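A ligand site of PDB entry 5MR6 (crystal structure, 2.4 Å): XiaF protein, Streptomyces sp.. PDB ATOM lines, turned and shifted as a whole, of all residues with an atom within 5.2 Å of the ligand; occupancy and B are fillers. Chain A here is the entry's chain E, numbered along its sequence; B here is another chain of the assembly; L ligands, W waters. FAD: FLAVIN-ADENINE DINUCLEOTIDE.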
ATOM      1  N   TRP A 103      -1.033  -4.728   1.597  1.00  0.00           N
ATOM      2  CA  TRP A 103      -1.746  -5.128   2.796  1.00  0.00           C
ATOM      3  C   TRP A 103      -1.223  -4.427   4.047  1.00  0.00           C
ATOM      4  O   TRP A 103      -1.995  -3.999   4.900  1.00  0.00           O
ATOM      5  CB  TRP A 103      -1.651  -6.626   2.972  1.00  0.00           C
ATOM      6  CG  TRP A 103      -2.514  -7.122   4.051  1.00  0.00           C
ATOM      7  CD1 TRP A 103      -2.114  -7.475   5.294  1.00  0.00           C
ATOM      8  CD2 TRP A 103      -3.938  -7.317   4.025  1.00  0.00           C
ATOM      9  NE1 TRP A 103      -3.174  -7.864   6.038  1.00  0.00           N
ATOM     10  CE2 TRP A 103      -4.306  -7.786   5.291  1.00  0.00           C
ATOM     11  CE3 TRP A 103      -4.930  -7.131   3.055  1.00  0.00           C
ATOM     12  CZ2 TRP A 103      -5.621  -8.082   5.617  1.00  0.00           C
ATOM     13  CZ3 TRP A 103      -6.226  -7.428   3.377  1.00  0.00           C
ATOM     14  CH2 TRP A 103      -6.562  -7.899   4.647  1.00  0.00           C
ATOM     15  N   ASN A 107      -3.160  -1.678   6.413  1.00  0.00           N
ATOM     16  CA  ASN A 107      -3.309  -1.897   7.834  1.00  0.00           C
ATOM     17  C   ASN A 107      -2.789  -0.708   8.620  1.00  0.00           C
ATOM     18  O   ASN A 107      -3.410  -0.325   9.586  1.00  0.00           O
ATOM     19  CB  ASN A 107      -2.614  -3.186   8.256  1.00  0.00           C
ATOM     20  CG  ASN A 107      -2.592  -3.381   9.769  1.00  0.00           C
ATOM     21  OD1 ASN A 107      -1.702  -2.849  10.478  1.00  0.00           O
ATOM     22  ND2 ASN A 107      -3.568  -4.129  10.277  1.00  0.00           N
ATOM     23  N   SER A 137      -2.686  -2.903  14.713  1.00  0.00           N
ATOM     24  CA  SER A 137      -3.891  -3.023  15.517  1.00  0.00           C
ATOM     25  C   SER A 137      -4.398  -4.436  15.378  1.00  0.00           C
ATOM     26  O   SER A 137      -4.487  -4.952  14.261  1.00  0.00           O
ATOM     27  CB  SER A 137      -4.951  -1.997  15.087  1.00  0.00           C
ATOM     28  OG  SER A 137      -5.355  -2.172  13.738  1.00  0.00           O
ATOM     29  N   VAL A 138      -4.650  -5.078  16.512  1.00  0.00           N
ATOM     30  CA  VAL A 138      -5.175  -6.415  16.524  1.00  0.00           C
ATOM     31  C   VAL A 138      -6.366  -6.510  17.448  1.00  0.00           C
ATOM     32  O   VAL A 138      -6.303  -6.112  18.585  1.00  0.00           O
ATOM     33  CB  VAL A 138      -4.100  -7.542  16.681  1.00  0.00           C
ATOM     34  CG1 VAL A 138      -2.706  -7.019  16.870  1.00  0.00           C
ATOM     35  CG2 VAL A 138      -4.478  -8.563  17.708  1.00  0.00           C
ATOM     36  N   PHE A 139      -7.480  -6.950  16.876  1.00  0.00           N
ATOM     37  CA  PHE A 139      -8.751  -7.142  17.566  1.00  0.00           C
ATOM     38  C   PHE A 139      -9.026  -8.660  17.675  1.00  0.00           C
ATOM     39  O   PHE A 139     -10.037  -9.086  18.205  1.00  0.00           O
ATOM     40  CB  PHE A 139      -9.840  -6.481  16.727  1.00  0.00           C
ATOM     41  CG  PHE A 139      -9.855  -4.966  16.761  1.00  0.00           C
ATOM     42  CD1 PHE A 139      -8.688  -4.214  16.626  1.00  0.00           C
ATOM     43  CD2 PHE A 139     -11.063  -4.289  16.871  1.00  0.00           C
ATOM     44  CE1 PHE A 139      -8.732  -2.828  16.660  1.00  0.00           C
ATOM     45  CE2 PHE A 139     -11.099  -2.903  16.893  1.00  0.00           C
ATOM     46  CZ  PHE A 139      -9.940  -2.171  16.778  1.00  0.00           C
ATOM     47  N   ALA A 140      -8.070  -9.446  17.179  1.00  0.00           N
ATOM     48  CA  ALA A 140      -8.090 -10.906  17.102  1.00  0.00           C
ATOM     49  C   ALA A 140      -7.877 -11.649  18.412  1.00  0.00           C
ATOM     50  O   ALA A 140      -7.898 -12.882  18.418  1.00  0.00           O
ATOM     51  CB  ALA A 140      -7.033 -11.391  16.104  1.00  0.00           C
ATOM     52  N   ALA A 141      -7.590 -10.945  19.492  1.00  0.00           N
ATOM     53  CA  ALA A 141      -7.440 -11.553  20.799  1.00  0.00           C
ATOM     54  C   ALA A 141      -7.811 -10.517  21.781  1.00  0.00           C
ATOM     55  O   ALA A 141      -7.933  -9.333  21.463  1.00  0.00           O
ATOM     56  CB  ALA A 141      -6.013 -12.019  21.078  1.00  0.00           C
ATOM     57  N   TYR A 160      -1.878 -12.557  14.532  1.00  0.00           N
ATOM     58  CA  TYR A 160      -2.238 -11.767  13.343  1.00  0.00           C
ATOM     59  C   TYR A 160      -1.867 -10.262  13.429  1.00  0.00           C
ATOM     60  O   TYR A 160      -2.641  -9.390  13.062  1.00  0.00           O
ATOM     61  CB  TYR A 160      -3.721 -11.909  13.036  1.00  0.00           C
ATOM     62  CG  TYR A 160      -4.160 -13.243  12.522  1.00  0.00           C
ATOM     63  CD1 TYR A 160      -3.963 -13.593  11.178  1.00  0.00           C
ATOM     64  CD2 TYR A 160      -4.831 -14.146  13.354  1.00  0.00           C
ATOM     65  CE1 TYR A 160      -4.404 -14.817  10.670  1.00  0.00           C
ATOM     66  CE2 TYR A 160      -5.280 -15.370  12.858  1.00  0.00           C
ATOM     67  CZ  TYR A 160      -5.069 -15.711  11.531  1.00  0.00           C
ATOM     68  OH  TYR A 160      -5.523 -16.915  11.058  1.00  0.00           O
ATOM     69  N   GLY A 161      -0.671  -9.975  13.897  1.00  0.00           N
ATOM     70  CA  GLY A 161      -0.261  -8.576  14.062  1.00  0.00           C
ATOM     71  C   GLY A 161       0.404  -8.100  12.804  1.00  0.00           C
ATOM     72  O   GLY A 161       1.634  -8.067  12.715  1.00  0.00           O
ATOM     73  N   THR A 162      -0.398  -7.746  11.807  1.00  0.00           N
ATOM     74  CA  THR A 162       0.162  -7.281  10.537  1.00  0.00           C
ATOM     75  C   THR A 162       1.136  -6.134  10.700  1.00  0.00           C
ATOM     76  O   THR A 162       0.858  -5.144  11.378  1.00  0.00           O
ATOM     77  CB  THR A 162      -0.927  -6.926   9.531  1.00  0.00           C
ATOM     78  OG1 THR A 162      -1.667  -8.106   9.263  1.00  0.00           O
ATOM     79  CG2 THR A 162      -0.353  -6.502   8.236  1.00  0.00           C
ATOM     80  N   TRP A 202       4.044 -16.434  12.243  1.00  0.00           N
ATOM     81  CA  TRP A 202       3.398 -16.282  10.953  1.00  0.00           C
ATOM     82  C   TRP A 202       4.029 -17.205   9.909  1.00  0.00           C
ATOM     83  O   TRP A 202       5.019 -16.875   9.298  1.00  0.00           O
ATOM     84  CB  TRP A 202       3.449 -14.816  10.536  1.00  0.00           C
ATOM     85  CG  TRP A 202       2.704 -14.448   9.295  1.00  0.00           C
ATOM     86  CD1 TRP A 202       3.250 -13.967   8.161  1.00  0.00           C
ATOM     87  CD2 TRP A 202       1.304 -14.488   9.069  1.00  0.00           C
ATOM     88  NE1 TRP A 202       2.290 -13.714   7.228  1.00  0.00           N
ATOM     89  CE2 TRP A 202       1.082 -14.035   7.757  1.00  0.00           C
ATOM     90  CE3 TRP A 202       0.228 -14.877   9.836  1.00  0.00           C
ATOM     91  CZ2 TRP A 202      -0.178 -13.953   7.197  1.00  0.00           C
ATOM     92  CZ3 TRP A 202      -1.021 -14.796   9.283  1.00  0.00           C
ATOM     93  CH2 TRP A 202      -1.211 -14.336   7.976  1.00  0.00           C
ATOM     94  N   MET A 207       0.493 -14.070   1.605  1.00  0.00           N
ATOM     95  CA  MET A 207       0.714 -12.848   2.356  1.00  0.00           C
ATOM     96  C   MET A 207       1.865 -13.027   3.360  1.00  0.00           C
ATOM     97  O   MET A 207       1.818 -12.541   4.470  1.00  0.00           O
ATOM     98  CB  MET A 207      -0.563 -12.408   3.067  1.00  0.00           C
ATOM     99  CG  MET A 207      -1.590 -11.681   2.210  1.00  0.00           C
ATOM    100  SD  MET A 207      -0.960 -10.385   1.120  1.00  0.00           S
ATOM    101  CE  MET A 207      -2.484  -9.527   0.725  1.00  0.00           C
ATOM    102  N   THR A 210       3.780  -9.933   4.991  1.00  0.00           N
ATOM    103  CA  THR A 210       3.035  -9.087   5.890  1.00  0.00           C
ATOM    104  C   THR A 210       3.504  -9.231   7.324  1.00  0.00           C
ATOM    105  O   THR A 210       3.219  -8.375   8.119  1.00  0.00           O
ATOM    106  CB  THR A 210       1.514  -9.346   5.858  1.00  0.00           C
ATOM    107  OG1 THR A 210       1.228 -10.692   6.233  1.00  0.00           O
ATOM    108  CG2 THR A 210       0.976  -9.079   4.504  1.00  0.00           C
ATOM    109  N   SER A 212       2.573 -11.029   9.940  1.00  0.00           N
ATOM    110  CA  SER A 212       1.480 -10.972  10.895  1.00  0.00           C
ATOM    111  C   SER A 212       1.709 -11.913  12.090  1.00  0.00           C
ATOM    112  O   SER A 212       0.983 -12.881  12.318  1.00  0.00           O
ATOM    113  CB  SER A 212       0.176 -11.202  10.154  1.00  0.00           C
ATOM    114  OG  SER A 212       0.063 -10.283   9.048  1.00  0.00           O
ATOM    115  N   THR A 383      -5.518 -15.671   0.595  1.00  0.00           N
ATOM    116  CA  THR A 383      -5.222 -15.611   2.010  1.00  0.00           C
ATOM    117  C   THR A 383      -5.866 -14.403   2.663  1.00  0.00           C
ATOM    118  O   THR A 383      -6.510 -14.521   3.690  1.00  0.00           O
ATOM    119  CB  THR A 383      -3.699 -15.509   2.216  1.00  0.00           C
ATOM    120  OG1 THR A 383      -3.071 -16.691   1.689  1.00  0.00           O
ATOM    121  CG2 THR A 383      -3.345 -15.366   3.695  1.00  0.00           C
ATOM    122  N   ALA A 384      -5.676 -13.252   2.063  1.00  0.00           N
ATOM    123  CA  ALA A 384      -6.205 -11.998   2.606  1.00  0.00           C
ATOM    124  C   ALA A 384      -7.722 -11.896   2.581  1.00  0.00           C
ATOM    125  O   ALA A 384      -8.326 -11.280   3.442  1.00  0.00           O
ATOM    126  CB  ALA A 384      -5.613 -10.822   1.852  1.00  0.00           C
ATOM    127  N   ARG A 386      -9.897 -14.040   3.331  1.00  0.00           N
ATOM    128  CA  ARG A 386     -10.540 -14.734   4.462  1.00  0.00           C
ATOM    129  C   ARG A 386     -10.351 -14.021   5.775  1.00  0.00           C
ATOM    130  O   ARG A 386     -10.651 -14.567   6.831  1.00  0.00           O
ATOM    131  CB  ARG A 386     -10.066 -16.187   4.571  1.00  0.00           C
ATOM    132  CG  ARG A 386     -10.872 -17.131   3.696  1.00  0.00           C
ATOM    133  CD  ARG A 386     -10.604 -16.880   2.245  1.00  0.00           C
ATOM    134  NE  ARG A 386     -11.372 -17.737   1.377  1.00  0.00           N
ATOM    135  CZ  ARG A 386     -11.029 -18.010   0.131  1.00  0.00           C
ATOM    136  NH1 ARG A 386     -11.792 -18.791  -0.622  1.00  0.00           N
ATOM    137  NH2 ARG A 386      -9.923 -17.511  -0.402  1.00  0.00           N
ATOM    138  N   HIS A 387      -9.881 -12.800   5.728  1.00  0.00           N
ATOM    139  CA  HIS A 387      -9.863 -11.969   6.904  1.00  0.00           C
ATOM    140  C   HIS A 387     -11.294 -11.840   7.383  1.00  0.00           C
ATOM    141  O   HIS A 387     -12.190 -11.777   6.593  1.00  0.00           O
ATOM    142  CB  HIS A 387      -9.310 -10.612   6.532  1.00  0.00           C
ATOM    143  CG  HIS A 387      -9.108  -9.683   7.680  1.00  0.00           C
ATOM    144  ND1 HIS A 387     -10.150  -9.077   8.325  1.00  0.00           N
ATOM    145  CD2 HIS A 387      -7.980  -9.214   8.261  1.00  0.00           C
ATOM    146  CE1 HIS A 387      -9.689  -8.291   9.266  1.00  0.00           C
ATOM    147  NE2 HIS A 387      -8.370  -8.357   9.258  1.00  0.00           N
ATOM    148  N   ALA A 388     -11.480 -11.801   8.681  1.00  0.00           N
ATOM    149  CA  ALA A 388     -12.802 -11.786   9.298  1.00  0.00           C
ATOM    150  C   ALA A 388     -13.733 -10.669   8.869  1.00  0.00           C
ATOM    151  O   ALA A 388     -14.929 -10.869   8.762  1.00  0.00           O
ATOM    152  CB  ALA A 388     -12.644 -11.769  10.806  1.00  0.00           C
ATOM    153  N   MET A 389     -13.197  -9.477   8.636  1.00  0.00           N
ATOM    154  CA  MET A 389     -14.003  -8.350   8.226  1.00  0.00           C
ATOM    155  C   MET A 389     -14.411  -8.440   6.769  1.00  0.00           C
ATOM    156  O   MET A 389     -15.195  -7.655   6.318  1.00  0.00           O
ATOM    157  CB  MET A 389     -13.252  -7.071   8.517  1.00  0.00           C
ATOM    158  CG  MET A 389     -13.083  -6.844  10.013  1.00  0.00           C
ATOM    159  SD  MET A 389     -14.605  -6.684  10.928  1.00  0.00           S
ATOM    160  CE  MET A 389     -15.285  -5.250  10.092  1.00  0.00           C
ATOM    161  N   GLY B 283     -15.010 -21.192  15.313  1.00  0.00           N
ATOM    162  CA  GLY B 283     -16.062 -20.224  15.062  1.00  0.00           C
ATOM    163  C   GLY B 283     -15.863 -19.510  13.727  1.00  0.00           C
ATOM    164  O   GLY B 283     -14.977 -19.809  12.951  1.00  0.00           O
ATOM    165  N   ILE B 284     -16.749 -18.554  13.496  1.00  0.00           N
ATOM    166  CA  ILE B 284     -16.748 -17.711  12.315  1.00  0.00           C
ATOM    167  C   ILE B 284     -16.582 -16.275  12.802  1.00  0.00           C
ATOM    168  O   ILE B 284     -17.554 -15.616  13.203  1.00  0.00           O
ATOM    169  CB  ILE B 284     -18.037 -17.839  11.505  1.00  0.00           C
ATOM    170  CG1 ILE B 284     -18.250 -19.284  11.098  1.00  0.00           C
ATOM    171  CG2 ILE B 284     -17.949 -16.989  10.238  1.00  0.00           C
ATOM    172  CD1 ILE B 284     -19.672 -19.591  10.793  1.00  0.00           C
ATOM    173  N   ALA B 285     -15.347 -15.802  12.753  1.00  0.00           N
ATOM    174  CA  ALA B 285     -15.069 -14.432  13.154  1.00  0.00           C
ATOM    175  C   ALA B 285     -15.591 -13.465  12.125  1.00  0.00           C
ATOM    176  O   ALA B 285     -15.516 -13.730  10.919  1.00  0.00           O
ATOM    177  CB  ALA B 285     -13.595 -14.205  13.325  1.00  0.00           C
ATOM    178  N   PRO B 286     -16.090 -12.321  12.596  1.00  0.00           N
ATOM    179  CA  PRO B 286     -16.220 -11.858  13.985  1.00  0.00           C
ATOM    180  C   PRO B 286     -17.650 -11.980  14.453  1.00  0.00           C
ATOM    181  O   PRO B 286     -18.151 -11.126  15.185  1.00  0.00           O
ATOM    182  CB  PRO B 286     -15.867 -10.395  13.879  1.00  0.00           C
ATOM    183  CG  PRO B 286     -16.500 -10.023  12.577  1.00  0.00           C
ATOM    184  CD  PRO B 286     -16.391 -11.224  11.676  1.00  0.00           C
ATOM    185  N   SER B 287     -18.314 -13.039  14.004  1.00  0.00           N
ATOM    186  CA  SER B 287     -19.741 -13.154  14.267  1.00  0.00           C
ATOM    187  C   SER B 287     -19.965 -13.678  15.667  1.00  0.00           C
ATOM    188  O   SER B 287     -19.040 -14.081  16.355  1.00  0.00           O
ATOM    189  CB  SER B 287     -20.420 -14.072  13.238  1.00  0.00           C
ATOM    190  OG  SER B 287     -20.010 -15.402  13.405  1.00  0.00           O
ATOM    191  N   ALA B 365      -9.360 -18.083   7.700  1.00  0.00           N
ATOM    192  CA  ALA B 365      -7.968 -17.696   7.486  1.00  0.00           C
ATOM    193  C   ALA B 365      -6.951 -18.738   7.903  1.00  0.00           C
ATOM    194  O   ALA B 365      -5.882 -18.816   7.318  1.00  0.00           O
ATOM    195  CB  ALA B 365      -7.689 -16.396   8.189  1.00  0.00           C
ATOM    196  N   ALA B 366      -7.289 -19.541   8.902  1.00  0.00           N
ATOM    197  CA  ALA B 366      -6.432 -20.584   9.399  1.00  0.00           C
ATOM    198  C   ALA B 366      -6.094 -21.626   8.351  1.00  0.00           C
ATOM    199  O   ALA B 366      -5.121 -22.363   8.475  1.00  0.00           O
ATOM    200  CB  ALA B 366      -7.097 -21.267  10.565  1.00  0.00           C
HETATM  201  PA  FAD L   1     -10.188 -16.310  15.648  1.00  0.00           P
HETATM  202  O1A FAD L   1      -8.896 -15.817  15.182  1.00  0.00           O
HETATM  203  O2A FAD L   1     -10.115 -17.574  16.337  1.00  0.00           O
HETATM  204  O5B FAD L   1     -10.770 -15.153  16.490  1.00  0.00           O
HETATM  205  C5B FAD L   1     -10.810 -15.199  17.890  1.00  0.00           C
HETATM  206  C4B FAD L   1     -11.707 -14.086  18.370  1.00  0.00           C
HETATM  207  O4B FAD L   1     -11.331 -12.860  17.811  1.00  0.00           O
HETATM  208  C3B FAD L   1     -13.150 -14.259  18.014  1.00  0.00           C
HETATM  209  O3B FAD L   1     -13.781 -13.832  19.186  1.00  0.00           O
HETATM  210  C2B FAD L   1     -13.438 -13.238  16.965  1.00  0.00           C
HETATM  211  O2B FAD L   1     -14.772 -12.771  17.026  1.00  0.00           O
HETATM  212  C1B FAD L   1     -12.461 -12.149  17.338  1.00  0.00           C
HETATM  213  N9A FAD L   1     -12.003 -11.380  16.173  1.00  0.00           N
HETATM  214  C8A FAD L   1     -11.163 -11.872  15.274  1.00  0.00           C
HETATM  215  N7A FAD L   1     -10.909 -10.975  14.335  1.00  0.00           N
HETATM  216  C5A FAD L   1     -11.597  -9.892  14.634  1.00  0.00           C
HETATM  217  C6A FAD L   1     -11.750  -8.576  14.043  1.00  0.00           C
HETATM  218  N6A FAD L   1     -11.115  -8.292  12.913  1.00  0.00           N
HETATM  219  N1A FAD L   1     -12.557  -7.705  14.658  1.00  0.00           N
HETATM  220  C2A FAD L   1     -13.195  -8.018  15.787  1.00  0.00           C
HETATM  221  N3A FAD L   1     -13.095  -9.189  16.364  1.00  0.00           N
HETATM  222  C4A FAD L   1     -12.327 -10.151  15.853  1.00  0.00           C
HETATM  223  N1  FAD L   1      -6.701  -9.296  12.562  1.00  0.00           N
HETATM  224  C2  FAD L   1      -6.337  -8.222  13.209  1.00  0.00           C
HETATM  225  O2  FAD L   1      -6.958  -7.879  14.193  1.00  0.00           O
HETATM  226  N3  FAD L   1      -5.318  -7.482  12.886  1.00  0.00           N
HETATM  227  C4  FAD L   1      -4.592  -7.750  11.836  1.00  0.00           C
HETATM  228  O4  FAD L   1      -3.676  -7.036  11.572  1.00  0.00           O
HETATM  229  C4X FAD L   1      -4.938  -8.922  11.049  1.00  0.00           C
HETATM  230  N5  FAD L   1      -4.239  -9.257   9.990  1.00  0.00           N
HETATM  231  C5X FAD L   1      -4.572 -10.333   9.297  1.00  0.00           C
HETATM  232  C6  FAD L   1      -3.839 -10.629   8.184  1.00  0.00           C
HETATM  233  C7  FAD L   1      -4.126 -11.715   7.410  1.00  0.00           C
HETATM  234  C7M FAD L   1      -3.285 -11.996   6.217  1.00  0.00           C
HETATM  235  C8  FAD L   1      -5.284 -12.556   7.794  1.00  0.00           C
HETATM  236  C8M FAD L   1      -5.607 -13.738   6.972  1.00  0.00           C
HETATM  237  C9  FAD L   1      -6.047 -12.258   8.903  1.00  0.00           C
HETATM  238  C9A FAD L   1      -5.741 -11.173   9.673  1.00  0.00           C
HETATM  239  N10 FAD L   1      -6.488 -10.806  10.793  1.00  0.00           N
HETATM  240  C10 FAD L   1      -6.069  -9.707  11.502  1.00  0.00           C
HETATM  241  C1' FAD L   1      -7.529 -11.679  11.266  1.00  0.00           C
HETATM  242  C2' FAD L   1      -9.019 -11.573  11.379  1.00  0.00           C
HETATM  243  O2' FAD L   1      -9.366 -10.596  12.292  1.00  0.00           O
HETATM  244  C3' FAD L   1      -9.433 -12.899  11.991  1.00  0.00           C
HETATM  245  O3' FAD L   1      -8.766 -13.040  13.226  1.00  0.00           O
HETATM  246  C4' FAD L   1      -9.023 -14.094  11.167  1.00  0.00           C
HETATM  247  O4' FAD L   1      -9.619 -13.917   9.920  1.00  0.00           O
HETATM  248  C5' FAD L   1      -9.340 -15.474  11.718  1.00  0.00           C
HETATM  249  O5' FAD L   1     -10.639 -15.628  12.242  1.00  0.00           O
HETATM  250  P   FAD L   1     -11.092 -16.924  12.964  1.00  0.00           P
HETATM  251  O1P FAD L   1     -12.445 -17.170  12.516  1.00  0.00           O
HETATM  252  O2P FAD L   1     -10.051 -17.917  12.778  1.00  0.00           O
HETATM  253  O3P FAD L   1     -11.230 -16.414  14.458  1.00  0.00           O
HETATM  254  O   HOH W   1     -11.225 -16.098   8.805  1.00  0.00           O
HETATM  255  O   HOH W   2     -12.403 -20.064  16.603  1.00  0.00           O
HETATM  256  O   HOH W   3      -9.594 -19.397  10.498  1.00  0.00           O
HETATM  257  O   HOH W   4     -16.312 -15.073  16.361  1.00  0.00           O
HETATM  258  O   HOH W   5     -16.256  -6.563  15.019  1.00  0.00           O
HETATM  259  O   HOH W   6     -13.746  -5.314  14.195  1.00  0.00           O
HETATM  260  O   HOH W   7      -7.309 -18.418  12.745  1.00  0.00           O
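The side-chain hydroxyl (OG1) of Thr 162 is in hydrogen-bond range of a nitrogen (N5) of the ligand, 2.9 Å away. The backbone NH (N) of Ala 285 of chain B lies within hydrogen-bond range of an oxygen (O1P) of the ligand (3.2 Å). N of Ala 388 lies within hydrogen-bond range of O4' of the ligand (3.1 Å). N of Phe 139 sits at hydrogen-bond distance from O2 of the ligand (2.9 Å). O of Tyr 160 lies close to N3 of the ligand (3.3 Å). The backbone NH (N) of Thr 162 lies within hydrogen-bond range of an oxygen (O4) of the ligand, 3.4 Å away. The backbone carbonyl oxygen (O) of Ser 137 lies within hydrogen-bond range of a nitrogen (N3) of the ligand (3.0 Å). ND2 of Asn 107 lies within hydrogen-bond range of O4 of the ligand (3.2 Å). O4' of the ligand is in hydrogen-bond range of O of Arg 386 (3.3 Å).
The side-chain hydroxyl (OG1) of Thr 162 sits at hydrogen-bond distance from the side-chain hydroxyl (OG) of Ser 212 (2.8 Å). The indole nitrogen (NE1) of Trp 202 sits at hydrogen-bond distance from the backbone carbonyl oxygen (O) of Met 207 (3.0 Å). The indole nitrogen (NE1) of Trp 202 is in hydrogen-bond range of the side-chain hydroxyl (OG1) of Thr 210 (3.4 Å). The backbone NH (N) of Met 389 lies within hydrogen-bond range of a ring nitrogen (ND1) of His 387, at 3.1 Å.
The backbone carbonyl oxygen (O) of Ala 140 lies close to an oxygen (O4B) of the ligand. A ring nitrogen (NE2) of His 387 lies close to a nitrogen (N10) of the ligand (3.4 Å). Trp 103 touches the ligand (NE1 to C6, 3.6 Å). CA of Val 138 touches O2 of the ligand, at 3.3 Å. Trp 202 touches the ligand. Thr 383 touches the ligand. Met 389 touches the ligand (CG to N6A, 3.8 Å). O of Gly 283 of chain B touches O1P of the ligand, 3.7 Å away. Pro 286 of chain B touches the ligand (CA to O2B, 3.5 Å). CB of Ala 365 of chain B touches O4' of the ligand, at 3.6 Å. Within 4 Å of the ligand: Trp 103, Asn 107, Ser 137, Val 138, Phe 139, Ala 140, Tyr 160, Thr 162, Trp 202, Thr 383, Arg 386, His 387, Ala 388, Met 389, Gly 283 of chain B, Ala 285 of chain B, Pro 286 of chain B and Ala 365 of chain B.
Water W6 bridges N1A of the ligand (2.7 Å) and SD of Met 389 (3.6 Å). Water W3 lies within hydrogen-bond range of O2P of the ligand, N of Ala 366 of chain B and N of Ala 365 of chain B. Water W7 lies within hydrogen-bond range of O2P of the ligand (2.8 Å) and OH of Tyr 160 (2.9 Å). Water W4 lies within hydrogen-bond range of O2B of the ligand (2.8 Å), O of Ser 287 of chain B (2.9 Å) and O of Ile 284 of chain B (3.4 Å). Water W1 lies within hydrogen-bond range of O of Arg 386 (2.6 Å), O4' of the ligand (2.9 Å) and N of Ala 365 of chain B (2.9 Å). Water W2 lies within hydrogen-bond range of the backbone NH (N) of Gly 283 of chain B (3.1 Å) and an oxygen (O2A) of the ligand (3.4 Å).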
